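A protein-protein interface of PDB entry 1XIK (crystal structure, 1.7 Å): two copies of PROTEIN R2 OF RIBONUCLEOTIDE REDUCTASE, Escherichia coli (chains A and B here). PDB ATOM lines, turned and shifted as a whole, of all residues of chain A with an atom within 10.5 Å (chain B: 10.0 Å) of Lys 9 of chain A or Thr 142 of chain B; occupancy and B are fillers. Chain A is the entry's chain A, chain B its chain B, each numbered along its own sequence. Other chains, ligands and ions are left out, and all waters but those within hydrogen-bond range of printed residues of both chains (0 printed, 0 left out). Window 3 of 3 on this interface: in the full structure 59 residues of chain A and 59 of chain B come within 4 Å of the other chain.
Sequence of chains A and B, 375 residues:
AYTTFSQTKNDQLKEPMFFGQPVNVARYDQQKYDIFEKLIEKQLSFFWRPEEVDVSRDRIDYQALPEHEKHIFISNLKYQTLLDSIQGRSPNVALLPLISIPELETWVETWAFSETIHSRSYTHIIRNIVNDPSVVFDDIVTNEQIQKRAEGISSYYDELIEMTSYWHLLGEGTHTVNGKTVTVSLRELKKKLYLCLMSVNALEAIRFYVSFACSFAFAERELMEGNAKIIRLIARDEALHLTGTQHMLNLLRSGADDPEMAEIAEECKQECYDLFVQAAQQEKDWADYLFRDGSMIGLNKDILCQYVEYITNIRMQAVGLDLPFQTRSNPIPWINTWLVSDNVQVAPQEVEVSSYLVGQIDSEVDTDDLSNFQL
Hydrophobic or aromatic side chains of chain A within 4 Å of the printed part of chain B: Val 25.
Of the 17 printed residues of chain B, 6 touch a printed residue of chain A.
Hydrophobic or aromatic side chains of chain B within 4 Å of the printed part of chain A: Phe 137 and Val 141.
Along chain B the printed residues that touch a printed residue of chain A span positions 134 to 147.
Among the printed residues, Asp or Glu carboxylates within 4 Å of a Lys or Arg side-chain nitrogen of the other chain: Arg 27 of chain A with Asp 138 of chain B.
Thr 142 of chain B touches just one residue of chain A: Lys 9 (3.9 Å).
Thr 8 of chain A touches one residue of chain B.
Asn 10 of chain A touches none of the printed residues of chain B.
Val 141 of chain B touches just these residues of chain A: Ser 6, Gln 7, Thr 8, Lys 9, Asn 24 and Val 25.
No residue of chain A comes within 4 Å of Asn 143 of chain B.
Of the printed residues of chain B, Asn 24 of chain A touches Val 141.
Of the printed residues of chain B, Gln 7 of chain A touches Val 141 and Gln 147.
Of the printed residues of chain A, Ser 134 of chain B touches Arg 27 (3.1 Å).
Phe 5 of chain A touches none of the printed residues of chain B.
The nearest residue of chain B that does not touch Lys 9 of chain A is Asp 139 of chain B (5.7 Å).
The nearest residue of chain A that does not touch Thr 142 of chain B is Gln 7 of chain A (4.2 Å).
The nearest printed residue of chain B that does not touch Val 25 of chain A is Ile 140 of chain B (4.5 Å).
ND2 of Asn 24 of chain A is in hydrogen-bond range of O of Ser 6 of chain A.
The side-chain amide nitrogen (ND2) of Asn 24 of chain A sits at hydrogen-bond distance from the backbone carbonyl oxygen (O) of Thr 8 of chain A (3.0 Å).
The side-chain amide nitrogen (NE2) of Gln 12 of chain A is in hydrogen-bond range of the side-chain amide oxygen (OD1) of Asn 24 of chain A (3.5 Å).
The backbone carbonyl oxygen (O) of Val 25 of chain A lies within hydrogen-bond range of the side-chain amide nitrogen (NE2) of Gln 12 of chain A.
The backbone carbonyl oxygen (O) of Thr 142 of chain B lies close to the side-chain amide oxygen (OE1) of Gln 147 of chain B (2.8 Å).
The backbone carbonyl oxygen of Asn 143 of chain B sits close to the side-chain amide oxygen of Gln 147 of chain B.
No position is printed for both chains.
Among the printed residues, merely in contact across the chains: Arg 27 of chain A with Phe 137 of chain B (3.4 Å), Asn 24 of chain A with Val 141 of chain B (3.4 Å), Gln 7 of chain A with Val 141 of chain B (3.5 Å), Lys 9 of chain A with Asp 138 of chain B (3.5 Å), Val 25 of chain A with Val 141 of chain B (3.6 Å), Thr 8 of chain A with Val 141 of chain B (3.7 Å), Ser 6 of chain A with Val 141 of chain B (3.7 Å), Lys 9 of chain A with Thr 142 of chain B (3.9 Å), Lys 9 of chain A with Val 141 of chain B (3.9 Å) and Val 25 of chain A with Phe 137 of chain B (3.96 Å).
The side-chain amide oxygen (OE1) of Gln 7 of chain A sits at hydrogen-bond distance from the side-chain amide nitrogen (NE2) of Gln 147 of chain B, at 2.9 Å.
The guanidinium group (NH2) of Arg 27 of chain A sits at hydrogen-bond distance from the side-chain hydroxyl (OG) of Ser 134 of chain B, 3.1 Å away.
The guanidinium group of Arg 27 of chain A is in salt-bridge range of the side-chain carboxylate of Asp 138 of chain B, at 3.8 Å.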
ATOM      1  N   PHE A   5     -16.576 -21.219 -21.248  1.00  0.00           N
ATOM      2  CA  PHE A   5     -17.375 -22.461 -21.178  1.00  0.00           C
ATOM      3  C   PHE A   5     -18.223 -22.465 -19.930  1.00  0.00           C
ATOM      4  O   PHE A   5     -17.753 -22.913 -18.872  1.00  0.00           O
ATOM      5  CB  PHE A   5     -16.584 -23.777 -21.289  1.00  0.00           C
ATOM      6  CG  PHE A   5     -17.443 -24.972 -21.689  1.00  0.00           C
ATOM      7  CD1 PHE A   5     -17.630 -25.323 -23.027  1.00  0.00           C
ATOM      8  CD2 PHE A   5     -18.040 -25.772 -20.715  1.00  0.00           C
ATOM      9  CE1 PHE A   5     -18.377 -26.430 -23.408  1.00  0.00           C
ATOM     10  CE2 PHE A   5     -18.788 -26.850 -21.099  1.00  0.00           C
ATOM     11  CZ  PHE A   5     -18.961 -27.184 -22.446  1.00  0.00           C
ATOM     12  N   SER A   6     -19.438 -21.929 -20.055  1.00  0.00           N
ATOM     13  CA  SER A   6     -20.359 -21.819 -18.913  1.00  0.00           C
ATOM     14  C   SER A   6     -20.715 -23.205 -18.403  1.00  0.00           C
ATOM     15  O   SER A   6     -21.078 -24.146 -19.164  1.00  0.00           O
ATOM     16  CB  SER A   6     -21.632 -21.075 -19.334  1.00  0.00           C
ATOM     17  OG  SER A   6     -22.122 -21.601 -20.556  1.00  0.00           O
ATOM     18  N   GLN A   7     -20.628 -23.347 -17.097  1.00  0.00           N
ATOM     19  CA  GLN A   7     -20.862 -24.636 -16.486  1.00  0.00           C
ATOM     20  C   GLN A   7     -22.263 -25.085 -16.135  1.00  0.00           C
ATOM     21  O   GLN A   7     -22.495 -26.175 -15.611  1.00  0.00           O
ATOM     22  CB  GLN A   7     -19.996 -24.624 -15.248  1.00  0.00           C
ATOM     23  CG  GLN A   7     -18.519 -24.750 -15.648  1.00  0.00           C
ATOM     24  CD  GLN A   7     -18.143 -26.149 -16.184  1.00  0.00           C
ATOM     25  OE1 GLN A   7     -17.640 -26.995 -15.439  1.00  0.00           O
ATOM     26  NE2 GLN A   7     -18.324 -26.369 -17.487  1.00  0.00           N
ATOM     27  N   THR A   8     -23.200 -24.230 -16.450  1.00  0.00           N
ATOM     28  CA  THR A   8     -24.545 -24.623 -16.155  1.00  0.00           C
ATOM     29  C   THR A   8     -25.094 -25.312 -17.391  1.00  0.00           C
ATOM     30  O   THR A   8     -24.886 -24.885 -18.529  1.00  0.00           O
ATOM     31  CB  THR A   8     -25.329 -23.348 -15.874  1.00  0.00           C
ATOM     32  OG1 THR A   8     -24.735 -22.707 -14.736  1.00  0.00           O
ATOM     33  CG2 THR A   8     -26.813 -23.611 -15.627  1.00  0.00           C
ATOM     34  N   LYS A   9     -25.812 -26.403 -17.143  1.00  0.00           N
ATOM     35  CA  LYS A   9     -26.465 -27.136 -18.207  1.00  0.00           C
ATOM     36  C   LYS A   9     -27.727 -26.304 -18.452  1.00  0.00           C
ATOM     37  O   LYS A   9     -28.644 -26.319 -17.658  1.00  0.00           O
ATOM     38  CB  LYS A   9     -26.863 -28.522 -17.704  1.00  0.00           C
ATOM     39  CG  LYS A   9     -27.551 -29.403 -18.747  1.00  0.00           C
ATOM     40  CD  LYS A   9     -27.709 -30.829 -18.207  1.00  0.00           C
ATOM     41  CE  LYS A   9     -29.152 -31.145 -17.900  1.00  0.00           C
ATOM     42  NZ  LYS A   9     -29.800 -32.106 -18.847  1.00  0.00           N
ATOM     43  N   ASN A  10     -27.758 -25.558 -19.550  1.00  0.00           N
ATOM     44  CA  ASN A  10     -28.889 -24.682 -19.885  1.00  0.00           C
ATOM     45  C   ASN A  10     -29.550 -25.128 -21.163  1.00  0.00           C
ATOM     46  O   ASN A  10     -28.881 -25.703 -21.991  1.00  0.00           O
ATOM     47  CB  ASN A  10     -28.418 -23.230 -19.988  1.00  0.00           C
ATOM     48  CG  ASN A  10     -27.503 -22.966 -21.174  1.00  0.00           C
ATOM     49  OD1 ASN A  10     -26.666 -23.789 -21.525  1.00  0.00           O
ATOM     50  ND2 ASN A  10     -27.653 -21.799 -21.789  1.00  0.00           N
ATOM     51  N   ASP A  11     -30.848 -24.905 -21.342  1.00  0.00           N
ATOM     52  CA  ASP A  11     -31.532 -25.316 -22.570  1.00  0.00           C
ATOM     53  C   ASP A  11     -31.275 -24.170 -23.533  1.00  0.00           C
ATOM     54  O   ASP A  11     -31.838 -23.077 -23.412  1.00  0.00           O
ATOM     55  CB  ASP A  11     -33.044 -25.362 -22.305  1.00  0.00           C
ATOM     56  CG  ASP A  11     -33.863 -25.781 -23.509  1.00  0.00           C
ATOM     57  OD1 ASP A  11     -33.399 -25.641 -24.660  1.00  0.00           O
ATOM     58  OD2 ASP A  11     -35.006 -26.252 -23.291  1.00  0.00           O
ATOM     59  N   GLN A  12     -30.398 -24.415 -24.496  1.00  0.00           N
ATOM     60  CA  GLN A  12     -30.051 -23.373 -25.455  1.00  0.00           C
ATOM     61  C   GLN A  12     -31.239 -22.900 -26.325  1.00  0.00           C
ATOM     62  O   GLN A  12     -31.162 -21.851 -26.954  1.00  0.00           O
ATOM     63  CB  GLN A  12     -28.901 -23.903 -26.325  1.00  0.00           C
ATOM     64  CG  GLN A  12     -27.613 -24.118 -25.536  1.00  0.00           C
ATOM     65  CD  GLN A  12     -26.527 -24.766 -26.372  1.00  0.00           C
ATOM     66  OE1 GLN A  12     -26.830 -25.458 -27.313  1.00  0.00           O
ATOM     67  NE2 GLN A  12     -25.274 -24.491 -26.072  1.00  0.00           N
ATOM     68  N   LEU A  13     -32.304 -23.689 -26.418  1.00  0.00           N
ATOM     69  CA  LEU A  13     -33.452 -23.294 -27.225  1.00  0.00           C
ATOM     70  C   LEU A  13     -34.189 -22.140 -26.554  1.00  0.00           C
ATOM     71  O   LEU A  13     -35.027 -21.470 -27.172  1.00  0.00           O
ATOM     72  CB  LEU A  13     -34.456 -24.432 -27.300  1.00  0.00           C
ATOM     73  CG  LEU A  13     -33.803 -25.514 -28.134  1.00  0.00           C
ATOM     74  CD1 LEU A  13     -34.668 -26.707 -28.230  1.00  0.00           C
ATOM     75  CD2 LEU A  13     -33.453 -25.017 -29.526  1.00  0.00           C
ATOM     76  N   LYS A  14     -33.919 -21.934 -25.274  1.00  0.00           N
ATOM     77  CA  LYS A  14     -34.676 -20.922 -24.579  1.00  0.00           C
ATOM     78  C   LYS A  14     -33.909 -19.709 -24.216  1.00  0.00           C
ATOM     79  O   LYS A  14     -34.422 -18.840 -23.513  1.00  0.00           O
ATOM     80  CB  LYS A  14     -35.357 -21.539 -23.357  1.00  0.00           C
ATOM     81  CG  LYS A  14     -36.411 -22.542 -23.731  1.00  0.00           C
ATOM     82  CD  LYS A  14     -37.092 -23.109 -22.516  1.00  0.00           C
ATOM     83  CE  LYS A  14     -38.073 -24.209 -22.926  1.00  0.00           C
ATOM     84  NZ  LYS A  14     -37.980 -25.418 -22.037  1.00  0.00           N
ATOM     85  N   GLU A  15     -32.665 -19.634 -24.667  1.00  0.00           N
ATOM     86  CA  GLU A  15     -31.894 -18.433 -24.328  1.00  0.00           C
ATOM     87  C   GLU A  15     -32.296 -17.356 -25.350  1.00  0.00           C
ATOM     88  O   GLU A  15     -32.771 -17.663 -26.434  1.00  0.00           O
ATOM     89  CB  GLU A  15     -30.382 -18.679 -24.491  1.00  0.00           C
ATOM     90  CG  GLU A  15     -29.847 -19.768 -23.564  1.00  0.00           C
ATOM     91  CD  GLU A  15     -29.709 -19.293 -22.137  1.00  0.00           C
ATOM     92  OE1 GLU A  15     -29.488 -18.088 -21.949  1.00  0.00           O
ATOM     93  OE2 GLU A  15     -29.772 -20.071 -21.162  1.00  0.00           O
ATOM     94  N   GLN A  21     -27.042 -16.774 -21.051  1.00  0.00           N
ATOM     95  CA  GLN A  21     -25.827 -17.433 -20.515  1.00  0.00           C
ATOM     96  C   GLN A  21     -24.887 -17.650 -21.719  1.00  0.00           C
ATOM     97  O   GLN A  21     -25.347 -18.025 -22.785  1.00  0.00           O
ATOM     98  CB  GLN A  21     -26.243 -18.792 -19.900  1.00  0.00           C
ATOM     99  CG  GLN A  21     -25.096 -19.832 -19.801  1.00  0.00           C
ATOM    100  CD  GLN A  21     -25.496 -21.177 -19.209  1.00  0.00           C
ATOM    101  OE1 GLN A  21     -26.536 -21.289 -18.570  1.00  0.00           O
ATOM    102  NE2 GLN A  21     -24.679 -22.205 -19.439  1.00  0.00           N
ATOM    103  N   PRO A  22     -23.589 -17.408 -21.591  1.00  0.00           N
ATOM    104  CA  PRO A  22     -22.687 -17.586 -22.730  1.00  0.00           C
ATOM    105  C   PRO A  22     -22.782 -19.016 -23.235  1.00  0.00           C
ATOM    106  O   PRO A  22     -23.107 -19.918 -22.459  1.00  0.00           O
ATOM    107  CB  PRO A  22     -21.306 -17.223 -22.162  1.00  0.00           C
ATOM    108  CG  PRO A  22     -21.600 -16.270 -21.027  1.00  0.00           C
ATOM    109  CD  PRO A  22     -22.899 -16.805 -20.440  1.00  0.00           C
ATOM    110  N   VAL A  23     -22.640 -19.182 -24.547  1.00  0.00           N
ATOM    111  CA  VAL A  23     -22.752 -20.507 -25.166  1.00  0.00           C
ATOM    112  C   VAL A  23     -21.666 -21.493 -24.643  1.00  0.00           C
ATOM    113  O   VAL A  23     -20.493 -21.111 -24.539  1.00  0.00           O
ATOM    114  CB  VAL A  23     -22.677 -20.416 -26.699  1.00  0.00           C
ATOM    115  CG1 VAL A  23     -22.860 -21.793 -27.306  1.00  0.00           C
ATOM    116  CG2 VAL A  23     -23.814 -19.541 -27.197  1.00  0.00           C
ATOM    117  N   ASN A  24     -22.061 -22.715 -24.283  1.00  0.00           N
ATOM    118  CA  ASN A  24     -21.024 -23.631 -23.853  1.00  0.00           C
ATOM    119  C   ASN A  24     -20.810 -24.581 -25.037  1.00  0.00           C
ATOM    120  O   ASN A  24     -19.847 -24.446 -25.809  1.00  0.00           O
ATOM    121  CB  ASN A  24     -21.328 -24.287 -22.491  1.00  0.00           C
ATOM    122  CG  ASN A  24     -22.776 -24.768 -22.303  1.00  0.00           C
ATOM    123  OD1 ASN A  24     -23.468 -25.229 -23.214  1.00  0.00           O
ATOM    124  ND2 ASN A  24     -23.221 -24.683 -21.052  1.00  0.00           N
ATOM    125  N   VAL A  25     -21.731 -25.524 -25.224  1.00  0.00           N
ATOM    126  CA  VAL A  25     -21.603 -26.465 -26.289  1.00  0.00           C
ATOM    127  C   VAL A  25     -22.060 -25.917 -27.594  1.00  0.00           C
ATOM    128  O   VAL A  25     -23.156 -25.348 -27.703  1.00  0.00           O
ATOM    129  CB  VAL A  25     -22.588 -27.619 -26.082  1.00  0.00           C
ATOM    130  CG1 VAL A  25     -22.487 -28.698 -27.219  1.00  0.00           C
ATOM    131  CG2 VAL A  25     -22.319 -28.189 -24.739  1.00  0.00           C
ATOM    132  N   ARG A  27     -23.414 -27.101 -30.788  1.00  0.00           N
ATOM    133  CA  ARG A  27     -24.144 -28.191 -31.433  1.00  0.00           C
ATOM    134  C   ARG A  27     -24.999 -27.539 -32.520  1.00  0.00           C
ATOM    135  O   ARG A  27     -25.438 -26.399 -32.380  1.00  0.00           O
ATOM    136  CB  ARG A  27     -25.066 -28.887 -30.405  1.00  0.00           C
ATOM    137  CG  ARG A  27     -25.693 -27.893 -29.442  1.00  0.00           C
ATOM    138  CD  ARG A  27     -26.487 -28.523 -28.338  1.00  0.00           C
ATOM    139  NE  ARG A  27     -27.472 -29.450 -28.895  1.00  0.00           N
ATOM    140  CZ  ARG A  27     -28.325 -30.136 -28.136  1.00  0.00           C
ATOM    141  NH1 ARG A  27     -28.279 -30.001 -26.822  1.00  0.00           N
ATOM    142  NH2 ARG A  27     -29.196 -30.981 -28.665  1.00  0.00           N
ATOM    143  N   GLN A  30     -30.259 -28.694 -33.517  1.00  0.00           N
ATOM    144  CA  GLN A  30     -31.529 -28.046 -33.271  1.00  0.00           C
ATOM    145  C   GLN A  30     -31.117 -26.576 -33.227  1.00  0.00           C
ATOM    146  O   GLN A  30     -29.941 -26.263 -32.975  1.00  0.00           O
ATOM    147  CB  GLN A  30     -31.995 -28.515 -31.894  1.00  0.00           C
ATOM    148  CG  GLN A  30     -30.954 -28.266 -30.815  1.00  0.00           C
ATOM    149  CD  GLN A  30     -31.520 -28.508 -29.433  1.00  0.00           C
ATOM    150  OE1 GLN A  30     -31.096 -27.920 -28.412  1.00  0.00           O
ATOM    151  NE2 GLN A  30     -32.504 -29.392 -29.398  1.00  0.00           N
ATOM    152  N   LYS B  78     -17.439 -36.732 -27.028  1.00  0.00           N
ATOM    153  CA  LYS B  78     -17.905 -35.640 -26.170  1.00  0.00           C
ATOM    154  C   LYS B  78     -16.763 -34.704 -25.807  1.00  0.00           C
ATOM    155  O   LYS B  78     -16.889 -33.465 -25.788  1.00  0.00           O
ATOM    156  CB  LYS B  78     -18.514 -36.195 -24.893  1.00  0.00           C
ATOM    157  CG  LYS B  78     -19.906 -36.749 -25.145  1.00  0.00           C
ATOM    158  CD  LYS B  78     -20.483 -37.201 -23.840  1.00  0.00           C
ATOM    159  CE  LYS B  78     -21.787 -37.951 -24.043  1.00  0.00           C
ATOM    160  NZ  LYS B  78     -22.002 -38.810 -22.808  1.00  0.00           N
ATOM    161  N   LEU B  82     -16.266 -30.805 -26.799  1.00  0.00           N
ATOM    162  CA  LEU B  82     -15.945 -29.770 -25.825  1.00  0.00           C
ATOM    163  C   LEU B  82     -14.737 -28.933 -26.234  1.00  0.00           C
ATOM    164  O   LEU B  82     -14.748 -27.697 -26.249  1.00  0.00           O
ATOM    165  CB  LEU B  82     -15.725 -30.411 -24.472  1.00  0.00           C
ATOM    166  CG  LEU B  82     -15.280 -29.511 -23.333  1.00  0.00           C
ATOM    167  CD1 LEU B  82     -15.729 -30.028 -22.004  1.00  0.00           C
ATOM    168  CD2 LEU B  82     -13.795 -29.377 -23.427  1.00  0.00           C
ATOM    169  N   SER B 134     -29.621 -35.143 -28.377  1.00  0.00           N
ATOM    170  CA  SER B 134     -29.616 -34.437 -27.110  1.00  0.00           C
ATOM    171  C   SER B 134     -29.045 -35.253 -26.035  1.00  0.00           C
ATOM    172  O   SER B 134     -28.505 -34.723 -25.063  1.00  0.00           O
ATOM    173  CB  SER B 134     -30.999 -34.036 -26.685  1.00  0.00           C
ATOM    174  OG  SER B 134     -31.327 -32.945 -27.496  1.00  0.00           O
ATOM    175  N   VAL B 135     -29.189 -36.554 -26.224  1.00  0.00           N
ATOM    176  CA  VAL B 135     -28.623 -37.385 -25.172  1.00  0.00           C
ATOM    177  C   VAL B 135     -27.142 -37.148 -25.096  1.00  0.00           C
ATOM    178  O   VAL B 135     -26.605 -36.852 -24.042  1.00  0.00           O
ATOM    179  CB  VAL B 135     -28.889 -38.861 -25.262  1.00  0.00           C
ATOM    180  CG1 VAL B 135     -28.690 -39.391 -23.816  1.00  0.00           C
ATOM    181  CG2 VAL B 135     -30.308 -39.094 -25.727  1.00  0.00           C
ATOM    182  N   VAL B 136     -26.493 -37.127 -26.240  1.00  0.00           N
ATOM    183  CA  VAL B 136     -25.081 -36.819 -26.132  1.00  0.00           C
ATOM    184  C   VAL B 136     -24.765 -35.380 -25.722  1.00  0.00           C
ATOM    185  O   VAL B 136     -24.042 -35.114 -24.786  1.00  0.00           O
ATOM    186  CB  VAL B 136     -24.366 -37.122 -27.419  1.00  0.00           C
ATOM    187  CG1 VAL B 136     -22.885 -36.935 -27.229  1.00  0.00           C
ATOM    188  CG2 VAL B 136     -24.690 -38.512 -27.833  1.00  0.00           C
ATOM    189  N   PHE B 137     -25.255 -34.400 -26.470  1.00  0.00           N
ATOM    190  CA  PHE B 137     -24.935 -33.009 -26.175  1.00  0.00           C
ATOM    191  C   PHE B 137     -25.358 -32.566 -24.809  1.00  0.00           C
ATOM    192  O   PHE B 137     -24.698 -31.750 -24.177  1.00  0.00           O
ATOM    193  CB  PHE B 137     -25.634 -32.145 -27.209  1.00  0.00           C
ATOM    194  CG  PHE B 137     -25.072 -32.287 -28.605  1.00  0.00           C
ATOM    195  CD1 PHE B 137     -23.714 -32.102 -28.838  1.00  0.00           C
ATOM    196  CD2 PHE B 137     -25.890 -32.572 -29.694  1.00  0.00           C
ATOM    197  CE1 PHE B 137     -23.184 -32.186 -30.103  1.00  0.00           C
ATOM    198  CE2 PHE B 137     -25.368 -32.642 -30.980  1.00  0.00           C
ATOM    199  CZ  PHE B 137     -24.015 -32.445 -31.186  1.00  0.00           C
ATOM    200  N   ASP B 138     -26.468 -33.099 -24.322  1.00  0.00           N
ATOM    201  CA  ASP B 138     -26.854 -32.632 -23.005  1.00  0.00           C
ATOM    202  C   ASP B 138     -26.060 -33.167 -21.843  1.00  0.00           C
ATOM    203  O   ASP B 138     -26.408 -32.852 -20.714  1.00  0.00           O
ATOM    204  CB  ASP B 138     -28.355 -32.833 -22.753  1.00  0.00           C
ATOM    205  CG  ASP B 138     -29.206 -31.680 -23.321  1.00  0.00           C
ATOM    206  OD1 ASP B 138     -28.899 -30.510 -22.947  1.00  0.00           O
ATOM    207  OD2 ASP B 138     -30.123 -31.922 -24.154  1.00  0.00           O
ATOM    208  N   ASP B 139     -25.030 -33.969 -22.116  1.00  0.00           N
ATOM    209  CA  ASP B 139     -24.215 -34.593 -21.098  1.00  0.00           C
ATOM    210  C   ASP B 139     -22.782 -34.111 -21.070  1.00  0.00           C
ATOM    211  O   ASP B 139     -21.991 -34.455 -20.206  1.00  0.00           O
ATOM    212  CB  ASP B 139     -24.244 -36.119 -21.301  1.00  0.00           C
ATOM    213  CG  ASP B 139     -23.385 -36.875 -20.264  1.00  0.00           C
ATOM    214  OD1 ASP B 139     -23.497 -36.586 -19.044  1.00  0.00           O
ATOM    215  OD2 ASP B 139     -22.534 -37.706 -20.656  1.00  0.00           O
ATOM    216  N   ILE B 140     -22.394 -33.252 -21.984  1.00  0.00           N
ATOM    217  CA  ILE B 140     -21.014 -32.807 -21.946  1.00  0.00           C
ATOM    218  C   ILE B 140     -20.737 -31.809 -20.837  1.00  0.00           C
ATOM    219  O   ILE B 140     -19.750 -31.884 -20.092  1.00  0.00           O
ATOM    220  CB  ILE B 140     -20.712 -32.115 -23.279  1.00  0.00           C
ATOM    221  CG1 ILE B 140     -21.046 -33.051 -24.441  1.00  0.00           C
ATOM    222  CG2 ILE B 140     -19.319 -31.609 -23.307  1.00  0.00           C
ATOM    223  CD1 ILE B 140     -20.485 -32.630 -25.762  1.00  0.00           C
ATOM    224  N   VAL B 141     -21.649 -30.851 -20.728  1.00  0.00           N
ATOM    225  CA  VAL B 141     -21.459 -29.773 -19.767  1.00  0.00           C
ATOM    226  C   VAL B 141     -21.233 -30.218 -18.354  1.00  0.00           C
ATOM    227  O   VAL B 141     -20.397 -29.666 -17.643  1.00  0.00           O
ATOM    228  CB  VAL B 141     -22.646 -28.711 -19.803  1.00  0.00           C
ATOM    229  CG1 VAL B 141     -22.430 -27.595 -18.762  1.00  0.00           C
ATOM    230  CG2 VAL B 141     -22.764 -28.086 -21.200  1.00  0.00           C
ATOM    231  N   THR B 142     -22.052 -31.173 -17.941  1.00  0.00           N
ATOM    232  CA  THR B 142     -21.988 -31.606 -16.561  1.00  0.00           C
ATOM    233  C   THR B 142     -21.343 -32.965 -16.369  1.00  0.00           C
ATOM    234  O   THR B 142     -21.201 -33.362 -15.224  1.00  0.00           O
ATOM    235  CB  THR B 142     -23.371 -31.561 -15.876  1.00  0.00           C
ATOM    236  OG1 THR B 142     -24.341 -32.158 -16.747  1.00  0.00           O
ATOM    237  CG2 THR B 142     -23.760 -30.137 -15.550  1.00  0.00           C
ATOM    238  N   ASN B 143     -20.958 -33.634 -17.455  1.00  0.00           N
ATOM    239  CA  ASN B 143     -20.286 -34.923 -17.319  1.00  0.00           C
ATOM    240  C   ASN B 143     -19.029 -34.743 -16.443  1.00  0.00           C
ATOM    241  O   ASN B 143     -18.088 -34.011 -16.772  1.00  0.00           O
ATOM    242  CB  ASN B 143     -19.906 -35.501 -18.685  1.00  0.00           C
ATOM    243  CG  ASN B 143     -19.171 -36.827 -18.577  1.00  0.00           C
ATOM    244  OD1 ASN B 143     -18.076 -36.915 -18.010  1.00  0.00           O
ATOM    245  ND2 ASN B 143     -19.781 -37.867 -19.113  1.00  0.00           N
ATOM    246  N   GLU B 144     -19.014 -35.432 -15.308  1.00  0.00           N
ATOM    247  CA  GLU B 144     -17.916 -35.324 -14.344  1.00  0.00           C
ATOM    248  C   GLU B 144     -16.581 -35.674 -14.943  1.00  0.00           C
ATOM    249  O   GLU B 144     -15.559 -35.049 -14.650  1.00  0.00           O
ATOM    250  CB  GLU B 144     -18.159 -36.362 -13.257  1.00  0.00           C
ATOM    251  CG  GLU B 144     -17.640 -36.001 -11.879  1.00  0.00           C
ATOM    252  CD  GLU B 144     -17.889 -37.134 -10.871  1.00  0.00           C
ATOM    253  OE1 GLU B 144     -17.222 -38.189 -10.994  1.00  0.00           O
ATOM    254  OE2 GLU B 144     -18.775 -36.997  -9.976  1.00  0.00           O
ATOM    255  N   GLN B 145     -16.631 -36.720 -15.754  1.00  0.00           N
ATOM    256  CA  GLN B 145     -15.428 -37.209 -16.355  1.00  0.00           C
ATOM    257  C   GLN B 145     -14.886 -36.230 -17.350  1.00  0.00           C
ATOM    258  O   GLN B 145     -13.668 -36.060 -17.437  1.00  0.00           O
ATOM    259  CB  GLN B 145     -15.701 -38.573 -16.975  1.00  0.00           C
ATOM    260  CG  GLN B 145     -15.794 -39.627 -15.867  1.00  0.00           C
ATOM    261  CD  GLN B 145     -14.787 -39.359 -14.742  1.00  0.00           C
ATOM    262  OE1 GLN B 145     -15.114 -39.461 -13.555  1.00  0.00           O
ATOM    263  NE2 GLN B 145     -13.553 -39.028 -15.114  1.00  0.00           N
ATOM    264  N   ILE B 146     -15.783 -35.571 -18.080  1.00  0.00           N
ATOM    265  CA  ILE B 146     -15.293 -34.630 -19.055  1.00  0.00           C
ATOM    266  C   ILE B 146     -14.823 -33.353 -18.428  1.00  0.00           C
ATOM    267  O   ILE B 146     -13.852 -32.816 -18.878  1.00  0.00           O
ATOM    268  CB  ILE B 146     -16.319 -34.300 -20.111  1.00  0.00           C
ATOM    269  CG1 ILE B 146     -17.026 -35.556 -20.612  1.00  0.00           C
ATOM    270  CG2 ILE B 146     -15.734 -33.350 -21.131  1.00  0.00           C
ATOM    271  CD1 ILE B 146     -16.540 -36.105 -21.920  1.00  0.00           C
ATOM    272  N   GLN B 147     -15.469 -32.850 -17.391  1.00  0.00           N
ATOM    273  CA  GLN B 147     -15.006 -31.588 -16.812  1.00  0.00           C
ATOM    274  C   GLN B 147     -13.681 -31.808 -16.156  1.00  0.00           C
ATOM    275  O   GLN B 147     -12.850 -30.908 -16.047  1.00  0.00           O
ATOM    276  CB  GLN B 147     -15.974 -31.061 -15.754  1.00  0.00           C
ATOM    277  CG  GLN B 147     -17.441 -31.094 -16.128  1.00  0.00           C
ATOM    278  CD  GLN B 147     -18.343 -30.861 -14.912  1.00  0.00           C
ATOM    279  OE1 GLN B 147     -18.983 -31.780 -14.395  1.00  0.00           O
ATOM    280  NE2 GLN B 147     -18.399 -29.614 -14.455  1.00  0.00           N
ATOM    281  N   LYS B 148     -13.511 -33.031 -15.680  1.00  0.00           N
ATOM    282  CA  LYS B 148     -12.247 -33.370 -15.010  1.00  0.00           C
ATOM    283  C   LYS B 148     -11.101 -33.395 -16.056  1.00  0.00           C
ATOM    284  O   LYS B 148     -10.042 -32.781 -15.874  1.00  0.00           O
ATOM    285  CB  LYS B 148     -12.321 -34.730 -14.276  1.00  0.00           C
ATOM    286  CG  LYS B 148     -12.664 -34.678 -12.779  1.00  0.00           C
ATOM    287  CD  LYS B 148     -13.134 -36.051 -12.244  1.00  0.00           C
ATOM    288  CE  LYS B 148     -14.226 -35.982 -11.151  1.00  0.00           C
ATOM    289  NZ  LYS B 148     -14.305 -37.231 -10.310  1.00  0.00           N
